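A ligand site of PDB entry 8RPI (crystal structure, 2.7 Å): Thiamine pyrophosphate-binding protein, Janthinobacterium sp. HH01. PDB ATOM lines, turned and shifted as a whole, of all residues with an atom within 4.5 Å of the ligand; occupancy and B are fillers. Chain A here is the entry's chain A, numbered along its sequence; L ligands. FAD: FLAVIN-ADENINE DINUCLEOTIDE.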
ATOM      1  N   ASP A  95      -4.518 -15.194 -29.774  1.00  0.00           N
ATOM      2  CA  ASP A  95      -4.948 -15.835 -28.536  1.00  0.00           C
ATOM      3  C   ASP A  95      -6.323 -15.380 -28.055  1.00  0.00           C
ATOM      4  O   ASP A  95      -6.756 -15.777 -26.978  1.00  0.00           O
ATOM      5  CB  ASP A  95      -3.904 -15.592 -27.434  1.00  0.00           C
ATOM      6  CG  ASP A  95      -2.676 -16.464 -27.595  1.00  0.00           C
ATOM      7  OD1 ASP A  95      -2.835 -17.658 -27.932  1.00  0.00           O
ATOM      8  OD2 ASP A  95      -1.551 -15.968 -27.375  1.00  0.00           O
ATOM      9  N   SER A  96      -7.011 -14.549 -28.832  1.00  0.00           N
ATOM     10  CA  SER A  96      -8.384 -14.142 -28.520  1.00  0.00           C
ATOM     11  C   SER A  96      -8.454 -13.363 -27.209  1.00  0.00           C
ATOM     12  O   SER A  96      -9.371 -13.561 -26.403  1.00  0.00           O
ATOM     13  CB  SER A  96      -9.310 -15.351 -28.472  1.00  0.00           C
ATOM     14  OG  SER A  96      -9.120 -16.188 -29.595  1.00  0.00           O
ATOM     15  N   GLY A 161     -18.101 -11.353 -28.587  1.00  0.00           N
ATOM     16  CA  GLY A 161     -17.890 -12.608 -29.297  1.00  0.00           C
ATOM     17  C   GLY A 161     -16.539 -13.224 -29.017  1.00  0.00           C
ATOM     18  O   GLY A 161     -16.178 -13.486 -27.876  1.00  0.00           O
ATOM     19  N   ARG A 162     -15.777 -13.477 -30.085  1.00  0.00           N
ATOM     20  CA  ARG A 162     -14.418 -13.958 -29.929  1.00  0.00           C
ATOM     21  C   ARG A 162     -13.540 -12.755 -29.602  1.00  0.00           C
ATOM     22  O   ARG A 162     -13.336 -11.894 -30.465  1.00  0.00           O
ATOM     23  CB  ARG A 162     -13.924 -14.649 -31.197  1.00  0.00           C
ATOM     24  CG  ARG A 162     -12.533 -15.219 -31.045  1.00  0.00           C
ATOM     25  CD  ARG A 162     -12.066 -15.898 -32.308  1.00  0.00           C
ATOM     26  NE  ARG A 162     -10.723 -16.438 -32.153  1.00  0.00           N
ATOM     27  CZ  ARG A 162     -10.081 -17.126 -33.079  1.00  0.00           C
ATOM     28  NH1 ARG A 162     -10.617 -17.355 -34.268  1.00  0.00           N
ATOM     29  NH2 ARG A 162      -8.869 -17.609 -32.813  1.00  0.00           N
ATOM     30  N   PRO A 163     -13.024 -12.641 -28.383  1.00  0.00           N
ATOM     31  CA  PRO A 163     -12.313 -11.427 -27.998  1.00  0.00           C
ATOM     32  C   PRO A 163     -11.047 -11.238 -28.821  1.00  0.00           C
ATOM     33  O   PRO A 163     -10.564 -12.147 -29.497  1.00  0.00           O
ATOM     34  CB  PRO A 163     -11.976 -11.642 -26.517  1.00  0.00           C
ATOM     35  CG  PRO A 163     -12.874 -12.749 -26.064  1.00  0.00           C
ATOM     36  CD  PRO A 163     -13.080 -13.608 -27.269  1.00  0.00           C
ATOM     37  N   GLY A 222     -10.859 -25.682 -23.030  1.00  0.00           N
ATOM     38  CA  GLY A 222      -9.926 -24.687 -23.510  1.00  0.00           C
ATOM     39  C   GLY A 222     -10.218 -23.310 -22.924  1.00  0.00           C
ATOM     40  O   GLY A 222     -11.256 -23.082 -22.295  1.00  0.00           O
ATOM     41  N   ASN A 223      -9.288 -22.389 -23.173  1.00  0.00           N
ATOM     42  CA  ASN A 223      -9.336 -21.063 -22.567  1.00  0.00           C
ATOM     43  C   ASN A 223     -10.543 -20.255 -22.999  1.00  0.00           C
ATOM     44  O   ASN A 223     -10.870 -19.261 -22.352  1.00  0.00           O
ATOM     45  CB  ASN A 223      -8.061 -20.286 -22.890  1.00  0.00           C
ATOM     46  CG  ASN A 223      -8.021 -18.946 -22.197  1.00  0.00           C
ATOM     47  OD1 ASN A 223      -8.395 -18.822 -21.029  1.00  0.00           O
ATOM     48  ND2 ASN A 223      -7.586 -17.908 -22.922  1.00  0.00           N
ATOM     49  N   GLY A 224     -11.213 -20.647 -24.078  1.00  0.00           N
ATOM     50  CA  GLY A 224     -12.462 -20.001 -24.427  1.00  0.00           C
ATOM     51  C   GLY A 224     -13.505 -20.085 -23.334  1.00  0.00           C
ATOM     52  O   GLY A 224     -14.406 -19.228 -23.277  1.00  0.00           O
ATOM     53  N   LEU A 227     -12.554 -17.129 -21.037  1.00  0.00           N
ATOM     54  CA  LEU A 227     -12.931 -15.886 -21.690  1.00  0.00           C
ATOM     55  C   LEU A 227     -14.442 -15.670 -21.649  1.00  0.00           C
ATOM     56  O   LEU A 227     -14.909 -14.526 -21.641  1.00  0.00           O
ATOM     57  CB  LEU A 227     -12.434 -15.876 -23.134  1.00  0.00           C
ATOM     58  CG  LEU A 227     -10.923 -15.894 -23.357  1.00  0.00           C
ATOM     59  CD1 LEU A 227     -10.568 -16.218 -24.804  1.00  0.00           C
ATOM     60  CD2 LEU A 227     -10.304 -14.560 -22.946  1.00  0.00           C
ATOM     61  N   ALA A 228     -15.208 -16.755 -21.645  1.00  0.00           N
ATOM     62  CA  ALA A 228     -16.665 -16.671 -21.534  1.00  0.00           C
ATOM     63  C   ALA A 228     -17.128 -16.563 -20.087  1.00  0.00           C
ATOM     64  O   ALA A 228     -18.319 -16.330 -19.858  1.00  0.00           O
ATOM     65  CB  ALA A 228     -17.303 -17.902 -22.183  1.00  0.00           C
ATOM     66  N   SER A 248      -6.320 -27.888 -22.568  1.00  0.00           N
ATOM     67  CA  SER A 248      -5.316 -27.338 -23.463  1.00  0.00           C
ATOM     68  C   SER A 248      -4.255 -26.609 -22.660  1.00  0.00           C
ATOM     69  O   SER A 248      -4.412 -26.323 -21.476  1.00  0.00           O
ATOM     70  CB  SER A 248      -5.958 -26.372 -24.454  1.00  0.00           C
ATOM     71  OG  SER A 248      -6.416 -25.215 -23.778  1.00  0.00           O
ATOM     72  N   TRP A 249      -3.145 -26.285 -23.335  1.00  0.00           N
ATOM     73  CA  TRP A 249      -2.083 -25.552 -22.664  1.00  0.00           C
ATOM     74  C   TRP A 249      -2.538 -24.184 -22.174  1.00  0.00           C
ATOM     75  O   TRP A 249      -2.033 -23.691 -21.162  1.00  0.00           O
ATOM     76  CB  TRP A 249      -0.893 -25.402 -23.617  1.00  0.00           C
ATOM     77  CG  TRP A 249      -0.017 -26.614 -23.679  1.00  0.00           C
ATOM     78  CD1 TRP A 249      -0.316 -27.868 -23.226  1.00  0.00           C
ATOM     79  CD2 TRP A 249       1.297 -26.686 -24.231  1.00  0.00           C
ATOM     80  NE1 TRP A 249       0.744 -28.717 -23.457  1.00  0.00           N
ATOM     81  CE2 TRP A 249       1.739 -28.017 -24.076  1.00  0.00           C
ATOM     82  CE3 TRP A 249       2.148 -25.763 -24.846  1.00  0.00           C
ATOM     83  CZ2 TRP A 249       2.998 -28.442 -24.513  1.00  0.00           C
ATOM     84  CZ3 TRP A 249       3.387 -26.188 -25.268  1.00  0.00           C
ATOM     85  CH2 TRP A 249       3.807 -27.509 -25.094  1.00  0.00           C
ATOM     86  N   ALA A 250      -3.491 -23.564 -22.867  1.00  0.00           N
ATOM     87  CA  ALA A 250      -3.979 -22.252 -22.458  1.00  0.00           C
ATOM     88  C   ALA A 250      -4.996 -22.355 -21.324  1.00  0.00           C
ATOM     89  O   ALA A 250      -5.116 -21.426 -20.524  1.00  0.00           O
ATOM     90  CB  ALA A 250      -4.597 -21.525 -23.653  1.00  0.00           C
ATOM     91  N   GLY A 251      -5.713 -23.468 -21.237  1.00  0.00           N
ATOM     92  CA  GLY A 251      -6.729 -23.632 -20.206  1.00  0.00           C
ATOM     93  C   GLY A 251      -6.300 -24.514 -19.058  1.00  0.00           C
ATOM     94  O   GLY A 251      -7.147 -25.033 -18.315  1.00  0.00           O
ATOM     95  N   ALA A 266      -2.900 -33.062 -24.039  1.00  0.00           N
ATOM     96  CA  ALA A 266      -2.501 -33.882 -25.173  1.00  0.00           C
ATOM     97  C   ALA A 266      -2.126 -33.011 -26.362  1.00  0.00           C
ATOM     98  O   ALA A 266      -2.566 -31.861 -26.471  1.00  0.00           O
ATOM     99  CB  ALA A 266      -3.630 -34.841 -25.575  1.00  0.00           C
ATOM    100  N   GLY A 267      -1.296 -33.556 -27.237  1.00  0.00           N
ATOM    101  CA  GLY A 267      -0.939 -32.882 -28.470  1.00  0.00           C
ATOM    102  C   GLY A 267       0.443 -33.292 -28.949  1.00  0.00           C
ATOM    103  O   GLY A 267       0.976 -34.317 -28.538  1.00  0.00           O
ATOM    104  N   VAL A 268       1.004 -32.453 -29.819  1.00  0.00           N
ATOM    105  CA  VAL A 268       2.312 -32.730 -30.415  1.00  0.00           C
ATOM    106  C   VAL A 268       3.393 -32.739 -29.346  1.00  0.00           C
ATOM    107  O   VAL A 268       4.379 -33.486 -29.429  1.00  0.00           O
ATOM    108  CB  VAL A 268       2.619 -31.698 -31.520  1.00  0.00           C
ATOM    109  CG1 VAL A 268       4.070 -31.799 -31.983  1.00  0.00           C
ATOM    110  CG2 VAL A 268       1.663 -31.894 -32.690  1.00  0.00           C
ATOM    111  N   TYR A 269       3.263 -31.864 -28.345  1.00  0.00           N
ATOM    112  CA  TYR A 269       4.068 -31.901 -27.133  1.00  0.00           C
ATOM    113  C   TYR A 269       3.226 -32.328 -25.941  1.00  0.00           C
ATOM    114  O   TYR A 269       3.439 -31.866 -24.819  1.00  0.00           O
ATOM    115  CB  TYR A 269       4.726 -30.549 -26.864  1.00  0.00           C
ATOM    116  CG  TYR A 269       5.954 -30.273 -27.712  1.00  0.00           C
ATOM    117  CD1 TYR A 269       5.843 -29.668 -28.951  1.00  0.00           C
ATOM    118  CD2 TYR A 269       7.223 -30.602 -27.257  1.00  0.00           C
ATOM    119  CE1 TYR A 269       6.951 -29.409 -29.720  1.00  0.00           C
ATOM    120  CE2 TYR A 269       8.340 -30.343 -28.021  1.00  0.00           C
ATOM    121  CZ  TYR A 269       8.202 -29.737 -29.250  1.00  0.00           C
ATOM    122  OH  TYR A 269       9.301 -29.480 -30.023  1.00  0.00           O
ATOM    123  N   GLY A 270       2.253 -33.206 -26.177  1.00  0.00           N
ATOM    124  CA  GLY A 270       1.385 -33.667 -25.124  1.00  0.00           C
ATOM    125  C   GLY A 270       2.102 -34.610 -24.170  1.00  0.00           C
ATOM    126  O   GLY A 270       3.298 -34.903 -24.292  1.00  0.00           O
ATOM    127  N   GLY A 288     -14.562 -24.706 -25.956  1.00  0.00           N
ATOM    128  CA  GLY A 288     -13.691 -23.559 -25.782  1.00  0.00           C
ATOM    129  C   GLY A 288     -12.247 -23.796 -26.145  1.00  0.00           C
ATOM    130  O   GLY A 288     -11.375 -23.055 -25.696  1.00  0.00           O
ATOM    131  N   THR A 289     -11.956 -24.817 -26.957  1.00  0.00           N
ATOM    132  CA  THR A 289     -10.599 -25.078 -27.411  1.00  0.00           C
ATOM    133  C   THR A 289     -10.551 -25.065 -28.926  1.00  0.00           C
ATOM    134  O   THR A 289     -11.451 -25.580 -29.594  1.00  0.00           O
ATOM    135  CB  THR A 289     -10.072 -26.428 -26.896  1.00  0.00           C
ATOM    136  OG1 THR A 289      -8.756 -26.646 -27.409  1.00  0.00           O
ATOM    137  CG2 THR A 289     -10.981 -27.560 -27.324  1.00  0.00           C
ATOM    138  N   ARG A 290      -9.485 -24.482 -29.471  1.00  0.00           N
ATOM    139  CA  ARG A 290      -9.352 -24.257 -30.901  1.00  0.00           C
ATOM    140  C   ARG A 290      -8.963 -25.509 -31.669  1.00  0.00           C
ATOM    141  O   ARG A 290      -9.063 -25.517 -32.902  1.00  0.00           O
ATOM    142  CB  ARG A 290      -8.315 -23.156 -31.143  1.00  0.00           C
ATOM    143  CG  ARG A 290      -8.275 -22.616 -32.572  1.00  0.00           C
ATOM    144  CD  ARG A 290      -7.588 -21.256 -32.638  1.00  0.00           C
ATOM    145  NE  ARG A 290      -6.257 -21.267 -32.045  1.00  0.00           N
ATOM    146  CZ  ARG A 290      -5.134 -21.494 -32.705  1.00  0.00           C
ATOM    147  NH1 ARG A 290      -5.132 -21.745 -34.008  1.00  0.00           N
ATOM    148  NH2 ARG A 290      -3.974 -21.462 -32.052  1.00  0.00           N
ATOM    149  N   ALA A 292      -5.973 -26.663 -32.232  1.00  0.00           N
ATOM    150  CA  ALA A 292      -4.907 -26.181 -33.105  1.00  0.00           C
ATOM    151  C   ALA A 292      -4.014 -27.335 -33.556  1.00  0.00           C
ATOM    152  O   ALA A 292      -4.092 -28.448 -33.024  1.00  0.00           O
ATOM    153  CB  ALA A 292      -4.070 -25.134 -32.376  1.00  0.00           C
ATOM    154  N   PRO A 294      -0.834 -27.982 -33.046  1.00  0.00           N
ATOM    155  CA  PRO A 294      -0.092 -28.616 -31.927  1.00  0.00           C
ATOM    156  C   PRO A 294      -0.978 -29.441 -31.002  1.00  0.00           C
ATOM    157  O   PRO A 294      -0.443 -30.171 -30.165  1.00  0.00           O
ATOM    158  CB  PRO A 294       0.523 -27.424 -31.187  1.00  0.00           C
ATOM    159  CG  PRO A 294       0.481 -26.288 -32.204  1.00  0.00           C
ATOM    160  CD  PRO A 294      -0.751 -26.520 -32.991  1.00  0.00           C
ATOM    161  N   GLN A 295      -2.289 -29.357 -31.148  1.00  0.00           N
ATOM    162  CA  GLN A 295      -3.185 -30.126 -30.296  1.00  0.00           C
ATOM    163  C   GLN A 295      -3.614 -31.440 -30.922  1.00  0.00           C
ATOM    164  O   GLN A 295      -3.692 -32.457 -30.232  1.00  0.00           O
ATOM    165  CB  GLN A 295      -4.434 -29.299 -29.961  1.00  0.00           C
ATOM    166  CG  GLN A 295      -4.198 -28.116 -29.056  1.00  0.00           C
ATOM    167  CD  GLN A 295      -5.492 -27.421 -28.722  1.00  0.00           C
ATOM    168  OE1 GLN A 295      -5.958 -26.546 -29.454  1.00  0.00           O
ATOM    169  NE2 GLN A 295      -6.101 -27.823 -27.611  1.00  0.00           N
ATOM    170  N   ASP A 313     -17.534 -23.681 -30.022  1.00  0.00           N
ATOM    171  CA  ASP A 313     -16.669 -22.530 -30.226  1.00  0.00           C
ATOM    172  C   ASP A 313     -17.528 -21.355 -30.685  1.00  0.00           C
ATOM    173  O   ASP A 313     -18.414 -21.522 -31.515  1.00  0.00           O
ATOM    174  CB  ASP A 313     -15.581 -22.839 -31.260  1.00  0.00           C
ATOM    175  CG  ASP A 313     -14.514 -21.763 -31.318  1.00  0.00           C
ATOM    176  OD1 ASP A 313     -14.875 -20.564 -31.413  1.00  0.00           O
ATOM    177  OD2 ASP A 313     -13.315 -22.112 -31.284  1.00  0.00           O
ATOM    178  N   ILE A 314     -17.246 -20.176 -30.125  1.00  0.00           N
ATOM    179  CA  ILE A 314     -18.050 -18.990 -30.454  1.00  0.00           C
ATOM    180  C   ILE A 314     -17.747 -18.422 -31.827  1.00  0.00           C
ATOM    181  O   ILE A 314     -18.479 -17.544 -32.310  1.00  0.00           O
ATOM    182  CB  ILE A 314     -17.829 -17.906 -29.375  1.00  0.00           C
ATOM    183  CG1 ILE A 314     -18.985 -16.904 -29.394  1.00  0.00           C
ATOM    184  CG2 ILE A 314     -16.492 -17.202 -29.569  1.00  0.00           C
ATOM    185  CD1 ILE A 314     -18.934 -15.931 -28.257  1.00  0.00           C
ATOM    186  N   ASP A 315     -16.680 -18.888 -32.474  1.00  0.00           N
ATOM    187  CA  ASP A 315     -16.291 -18.434 -33.801  1.00  0.00           C
ATOM    188  C   ASP A 315     -16.740 -19.482 -34.815  1.00  0.00           C
ATOM    189  O   ASP A 315     -16.314 -20.637 -34.764  1.00  0.00           O
ATOM    190  CB  ASP A 315     -14.784 -18.229 -33.855  1.00  0.00           C
ATOM    191  CG  ASP A 315     -14.327 -17.493 -35.094  1.00  0.00           C
ATOM    192  OD1 ASP A 315     -14.924 -17.680 -36.170  1.00  0.00           O
ATOM    193  OD2 ASP A 315     -13.345 -16.718 -34.989  1.00  0.00           O
ATOM    194  N   GLU A 318     -13.896 -21.176 -36.810  1.00  0.00           N
ATOM    195  CA  GLU A 318     -13.139 -22.153 -36.035  1.00  0.00           C
ATOM    196  C   GLU A 318     -13.959 -23.394 -35.732  1.00  0.00           C
ATOM    197  O   GLU A 318     -13.399 -24.480 -35.558  1.00  0.00           O
ATOM    198  CB  GLU A 318     -12.642 -21.517 -34.726  1.00  0.00           C
ATOM    199  CG  GLU A 318     -11.714 -20.311 -34.884  1.00  0.00           C
ATOM    200  CD  GLU A 318     -10.325 -20.676 -35.362  1.00  0.00           C
ATOM    201  OE1 GLU A 318     -10.012 -21.886 -35.453  1.00  0.00           O
ATOM    202  OE2 GLU A 318      -9.538 -19.749 -35.641  1.00  0.00           O
ATOM    203  N   CYS A 332     -21.512 -21.486 -30.279  1.00  0.00           N
ATOM    204  CA  CYS A 332     -22.157 -20.986 -29.081  1.00  0.00           C
ATOM    205  C   CYS A 332     -21.092 -20.530 -28.095  1.00  0.00           C
ATOM    206  O   CYS A 332     -19.965 -21.028 -28.096  1.00  0.00           O
ATOM    207  CB  CYS A 332     -23.045 -22.061 -28.437  1.00  0.00           C
ATOM    208  SG  CYS A 332     -24.112 -21.473 -27.097  1.00  0.00           S
ATOM    209  N   ASP A 333     -21.463 -19.543 -27.278  1.00  0.00           N
ATOM    210  CA  ASP A 333     -20.606 -19.146 -26.166  1.00  0.00           C
ATOM    211  C   ASP A 333     -20.392 -20.326 -25.233  1.00  0.00           C
ATOM    212  O   ASP A 333     -21.313 -21.101 -24.957  1.00  0.00           O
ATOM    213  CB  ASP A 333     -21.228 -17.972 -25.416  1.00  0.00           C
ATOM    214  CG  ASP A 333     -20.365 -17.477 -24.265  1.00  0.00           C
ATOM    215  OD1 ASP A 333     -20.512 -18.008 -23.151  1.00  0.00           O
ATOM    216  OD2 ASP A 333     -19.529 -16.570 -24.482  1.00  0.00           O
ATOM    217  N   ALA A 334     -19.163 -20.464 -24.728  1.00  0.00           N
ATOM    218  CA  ALA A 334     -18.820 -21.635 -23.934  1.00  0.00           C
ATOM    219  C   ALA A 334     -19.636 -21.683 -22.652  1.00  0.00           C
ATOM    220  O   ALA A 334     -20.131 -22.747 -22.262  1.00  0.00           O
ATOM    221  CB  ALA A 334     -17.330 -21.633 -23.622  1.00  0.00           C
ATOM    222  N   LEU A 411       8.517 -22.901 -21.967  1.00  0.00           N
ATOM    223  CA  LEU A 411       7.206 -23.235 -22.502  1.00  0.00           C
ATOM    224  C   LEU A 411       6.970 -24.746 -22.474  1.00  0.00           C
ATOM    225  O   LEU A 411       5.936 -25.210 -21.989  1.00  0.00           O
ATOM    226  CB  LEU A 411       7.087 -22.706 -23.929  1.00  0.00           C
ATOM    227  CG  LEU A 411       5.861 -23.182 -24.736  1.00  0.00           C
ATOM    228  CD1 LEU A 411       4.599 -22.522 -24.221  1.00  0.00           C
ATOM    229  CD2 LEU A 411       6.056 -22.904 -26.206  1.00  0.00           C
ATOM    230  N   LEU A 412       7.932 -25.520 -22.983  1.00  0.00           N
ATOM    231  CA  LEU A 412       7.705 -26.955 -23.157  1.00  0.00           C
ATOM    232  C   LEU A 412       7.788 -27.690 -21.824  1.00  0.00           C
ATOM    233  O   LEU A 412       6.822 -28.335 -21.396  1.00  0.00           O
ATOM    234  CB  LEU A 412       8.726 -27.516 -24.153  1.00  0.00           C
ATOM    235  CG  LEU A 412       8.781 -26.828 -25.526  1.00  0.00           C
ATOM    236  CD1 LEU A 412       9.951 -27.353 -26.360  1.00  0.00           C
ATOM    237  CD2 LEU A 412       7.472 -26.981 -26.287  1.00  0.00           C
ATOM    238  N   THR A 430       0.563 -18.567 -26.959  1.00  0.00           N
ATOM    239  CA  THR A 430       0.716 -19.772 -27.759  1.00  0.00           C
ATOM    240  C   THR A 430       0.153 -19.632 -29.167  1.00  0.00           C
ATOM    241  O   THR A 430       0.628 -20.316 -30.076  1.00  0.00           O
ATOM    242  CB  THR A 430       0.030 -20.947 -27.053  1.00  0.00           C
ATOM    243  OG1 THR A 430      -1.190 -20.504 -26.456  1.00  0.00           O
ATOM    244  CG2 THR A 430       0.934 -21.516 -25.994  1.00  0.00           C
ATOM    245  N   GLY A 431      -0.817 -18.744 -29.371  1.00  0.00           N
ATOM    246  CA  GLY A 431      -1.320 -18.503 -30.713  1.00  0.00           C
ATOM    247  C   GLY A 431      -0.219 -18.070 -31.667  1.00  0.00           C
ATOM    248  O   GLY A 431      -0.069 -18.623 -32.755  1.00  0.00           O
ATOM    249  N   MET A 492      15.695 -25.099 -28.926  1.00  0.00           N
ATOM    250  CA  MET A 492      14.549 -25.611 -29.663  1.00  0.00           C
ATOM    251  C   MET A 492      14.844 -25.726 -31.157  1.00  0.00           C
ATOM    252  O   MET A 492      14.423 -26.701 -31.806  1.00  0.00           O
ATOM    253  CB  MET A 492      13.342 -24.696 -29.421  1.00  0.00           C
ATOM    254  CG  MET A 492      12.027 -25.298 -29.823  1.00  0.00           C
ATOM    255  SD  MET A 492      10.668 -24.573 -28.897  1.00  0.00           S
ATOM    256  CE  MET A 492       9.305 -25.358 -29.741  1.00  0.00           C
HETATM  257  PA  FAD L   1      -6.896 -20.859 -28.043  1.00  0.00           P
HETATM  258  O1A FAD L   1      -6.815 -19.426 -27.699  1.00  0.00           O
HETATM  259  O2A FAD L   1      -6.145 -21.252 -29.307  1.00  0.00           O
HETATM  260  O5B FAD L   1      -8.348 -21.303 -28.165  1.00  0.00           O
HETATM  261  C5B FAD L   1      -9.436 -20.423 -27.798  1.00  0.00           C
HETATM  262  C4B FAD L   1     -10.616 -20.862 -28.613  1.00  0.00           C
HETATM  263  O4B FAD L   1     -11.823 -20.549 -27.890  1.00  0.00           O
HETATM  264  C3B FAD L   1     -10.724 -20.167 -29.977  1.00  0.00           C
HETATM  265  O3B FAD L   1     -11.144 -21.070 -31.004  1.00  0.00           O
HETATM  266  C2B FAD L   1     -11.751 -19.067 -29.716  1.00  0.00           C
HETATM  267  O2B FAD L   1     -12.468 -18.705 -30.883  1.00  0.00           O
HETATM  268  C1B FAD L   1     -12.670 -19.758 -28.703  1.00  0.00           C
HETATM  269  N9A FAD L   1     -13.404 -18.838 -27.852  1.00  0.00           N
HETATM  270  C8A FAD L   1     -13.014 -17.585 -27.446  1.00  0.00           C
HETATM  271  N7A FAD L   1     -13.900 -16.978 -26.690  1.00  0.00           N
HETATM  272  C5A FAD L   1     -14.942 -17.884 -26.597  1.00  0.00           C
HETATM  273  C6A FAD L   1     -16.185 -17.842 -25.940  1.00  0.00           C
HETATM  274  N6A FAD L   1     -16.597 -16.797 -25.224  1.00  0.00           N
HETATM  275  N1A FAD L   1     -16.994 -18.919 -26.050  1.00  0.00           N
HETATM  276  C2A FAD L   1     -16.577 -19.960 -26.774  1.00  0.00           C
HETATM  277  N3A FAD L   1     -15.435 -20.115 -27.438  1.00  0.00           N
HETATM  278  C4A FAD L   1     -14.654 -19.038 -27.318  1.00  0.00           C
HETATM  279  N1  FAD L   1      -1.471 -27.163 -26.846  1.00  0.00           N
HETATM  280  C2  FAD L   1      -1.864 -28.389 -26.388  1.00  0.00           C
HETATM  281  O2  FAD L   1      -2.995 -28.585 -25.929  1.00  0.00           O
HETATM  282  N3  FAD L   1      -0.987 -29.457 -26.453  1.00  0.00           N
HETATM  283  C4  FAD L   1       0.305 -29.418 -26.936  1.00  0.00           C
HETATM  284  O4  FAD L   1       0.997 -30.427 -26.939  1.00  0.00           O
HETATM  285  C4X FAD L   1       0.716 -28.112 -27.418  1.00  0.00           C
HETATM  286  N5  FAD L   1       1.924 -27.981 -27.885  1.00  0.00           N
HETATM  287  C5X FAD L   1       2.315 -26.746 -28.339  1.00  0.00           C
HETATM  288  C6  FAD L   1       3.609 -26.600 -28.842  1.00  0.00           C
HETATM  289  C7  FAD L   1       4.067 -25.372 -29.315  1.00  0.00           C
HETATM  290  C7M FAD L   1       5.460 -25.265 -29.850  1.00  0.00           C
HETATM  291  C8  FAD L   1       3.212 -24.255 -29.278  1.00  0.00           C
HETATM  292  C8M FAD L   1       3.665 -22.909 -29.781  1.00  0.00           C
HETATM  293  C9  FAD L   1       1.916 -24.392 -28.772  1.00  0.00           C
HETATM  294  C9A FAD L   1       1.469 -25.628 -28.296  1.00  0.00           C
HETATM  295  N10 FAD L   1       0.168 -25.804 -27.776  1.00  0.00           N
HETATM  296  C10 FAD L   1      -0.241 -27.041 -27.331  1.00  0.00           C
HETATM  297  C1' FAD L   1      -0.787 -24.677 -27.721  1.00  0.00           C
HETATM  298  C2' FAD L   1      -1.904 -24.807 -28.766  1.00  0.00           C
HETATM  299  O2' FAD L   1      -1.342 -25.088 -30.054  1.00  0.00           O
HETATM  300  C3' FAD L   1      -2.691 -23.498 -28.844  1.00  0.00           C
HETATM  301  O3' FAD L   1      -1.798 -22.402 -29.025  1.00  0.00           O
HETATM  302  C4' FAD L   1      -3.586 -23.200 -27.636  1.00  0.00           C
HETATM  303  O4' FAD L   1      -2.787 -23.060 -26.461  1.00  0.00           O
HETATM  304  C5' FAD L   1      -4.642 -24.258 -27.406  1.00  0.00           C
HETATM  305  O5' FAD L   1      -5.398 -23.921 -26.233  1.00  0.00           O
HETATM  306  P   FAD L   1      -6.781 -23.190 -26.339  1.00  0.00           P
HETATM  307  O1P FAD L   1      -7.593 -23.903 -27.425  1.00  0.00           O
HETATM  308  O2P FAD L   1      -7.399 -23.082 -25.005  1.00  0.00           O
HETATM  309  O3P FAD L   1      -6.331 -21.742 -26.853  1.00  0.00           O
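OD2 of Asp 313 sits at hydrogen-bond distance from O3B of the ligand, at 2.4 Å.
An oxygen (O2P) of the ligand lies within hydrogen-bond range of the side-chain hydroxyl (OG) of Ser 248 (2.6 Å).
An oxygen (O2P) of the ligand lies within hydrogen-bond range of the backbone NH (N) of Asn 223.
The backbone NH (N) of Arg 290 is in hydrogen-bond range of an oxygen (O1P) of the ligand.
NE of Arg 290 lies within salt-bridge range of O2A of the ligand, at 2.7 Å.
The backbone carbonyl oxygen of Ala 266 is in hydrogen-bond range of a nitrogen (N3) of the ligand (2.9 Å).
A nitrogen (N1A) of the ligand sits at hydrogen-bond distance from the backbone NH (N) of Ala 334 (3.0 Å).
The side-chain hydroxyl (OG1) of Thr 289 sits at hydrogen-bond distance from an oxygen (O1P) of the ligand (3.0 Å).
O of Thr 430 lies close to O3' of the ligand (3.4 Å).
The side-chain hydroxyl of Thr 430 is in hydrogen-bond range of an oxygen (O4') of the ligand (3.0 Å).
The backbone NH (N) of Tyr 269 lies within hydrogen-bond range of an oxygen (O4) of the ligand (3.0 Å).
N6A of the ligand lies within hydrogen-bond range of OD2 of Asp 333.
The guanidinium group (NE) of Arg 162 lies within hydrogen-bond range of an oxygen (O2B) of the ligand, 3.1 Å away.
N of Gly 270 is in hydrogen-bond range of O4 of the ligand (3.1 Å).
The backbone NH (N) of Ile 314 lies within hydrogen-bond range of a nitrogen (N3A) of the ligand (3.2 Å).
The backbone NH (N) of Trp 249 lies within hydrogen-bond range of an oxygen (O2) of the ligand (3.5 Å).
The backbone NH (N) of Cys 332 lies within hydrogen-bond range of the backbone carbonyl oxygen (O) of Asp 313, at 3.3 Å.
The backbone NH (N) of Asp 315 sits at hydrogen-bond distance from the side-chain carboxylate (OD1) of Asp 313, 2.7 Å away.
The backbone NH (N) of Ala 250 lies close to the side-chain hydroxyl (OG) of Ser 248 (3.5 Å).
The side-chain hydroxyl (OG) of Ser 248 is in hydrogen-bond range of the backbone NH (N) of Gly 251 (3.2 Å).
The side-chain hydroxyl of Thr 289 lies within hydrogen-bond range of the side-chain amide nitrogen of Gln 295 (2.9 Å).
The backbone NH (N) of Thr 430 is in hydrogen-bond range of the side-chain carboxylate (OD2) of Asp 95, at 3.4 Å.
N of Val 268 lies within hydrogen-bond range of O of Pro 294, at 2.7 Å.
NH1 of Arg 162 is in salt-bridge range of OD2 of Asp 315 (2.9 Å).
O4B of the ligand sits close to O of Gly 288 (3.4 Å).
Merely in contact with the ligand: Asp 95 (3.7 Å), Ser 96 (3.9 Å), Pro 163 (3.5 Å), Gly 222 (3.3 Å), Gly 224 (3.5 Å), Leu 227 (3.9 Å), Ala 228 (3.3 Å), Ala 250 (3.5 Å), Gly 267 (3.5 Å), Val 268 (3.5 Å), Ala 292 (3.6 Å), Pro 294 (3.1 Å), Gln 295 (3.3 Å), Asp 315 (3.8 Å), Glu 318 (3.99 Å), Cys 332 (3.8 Å), Gly 431 (3.8 Å) and Met 492 (3.8 Å).
Hydrophobic or aromatic side chains within 4 Å of the ligand: Pro 163, Leu 227, Ala 228, Trp 249, Ala 250, Tyr 269, Ala 292, Pro 294, Ile 314, Ala 334 and Met 492.
Of the 37 residues printed, 33 come within 4 Å of the ligand.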
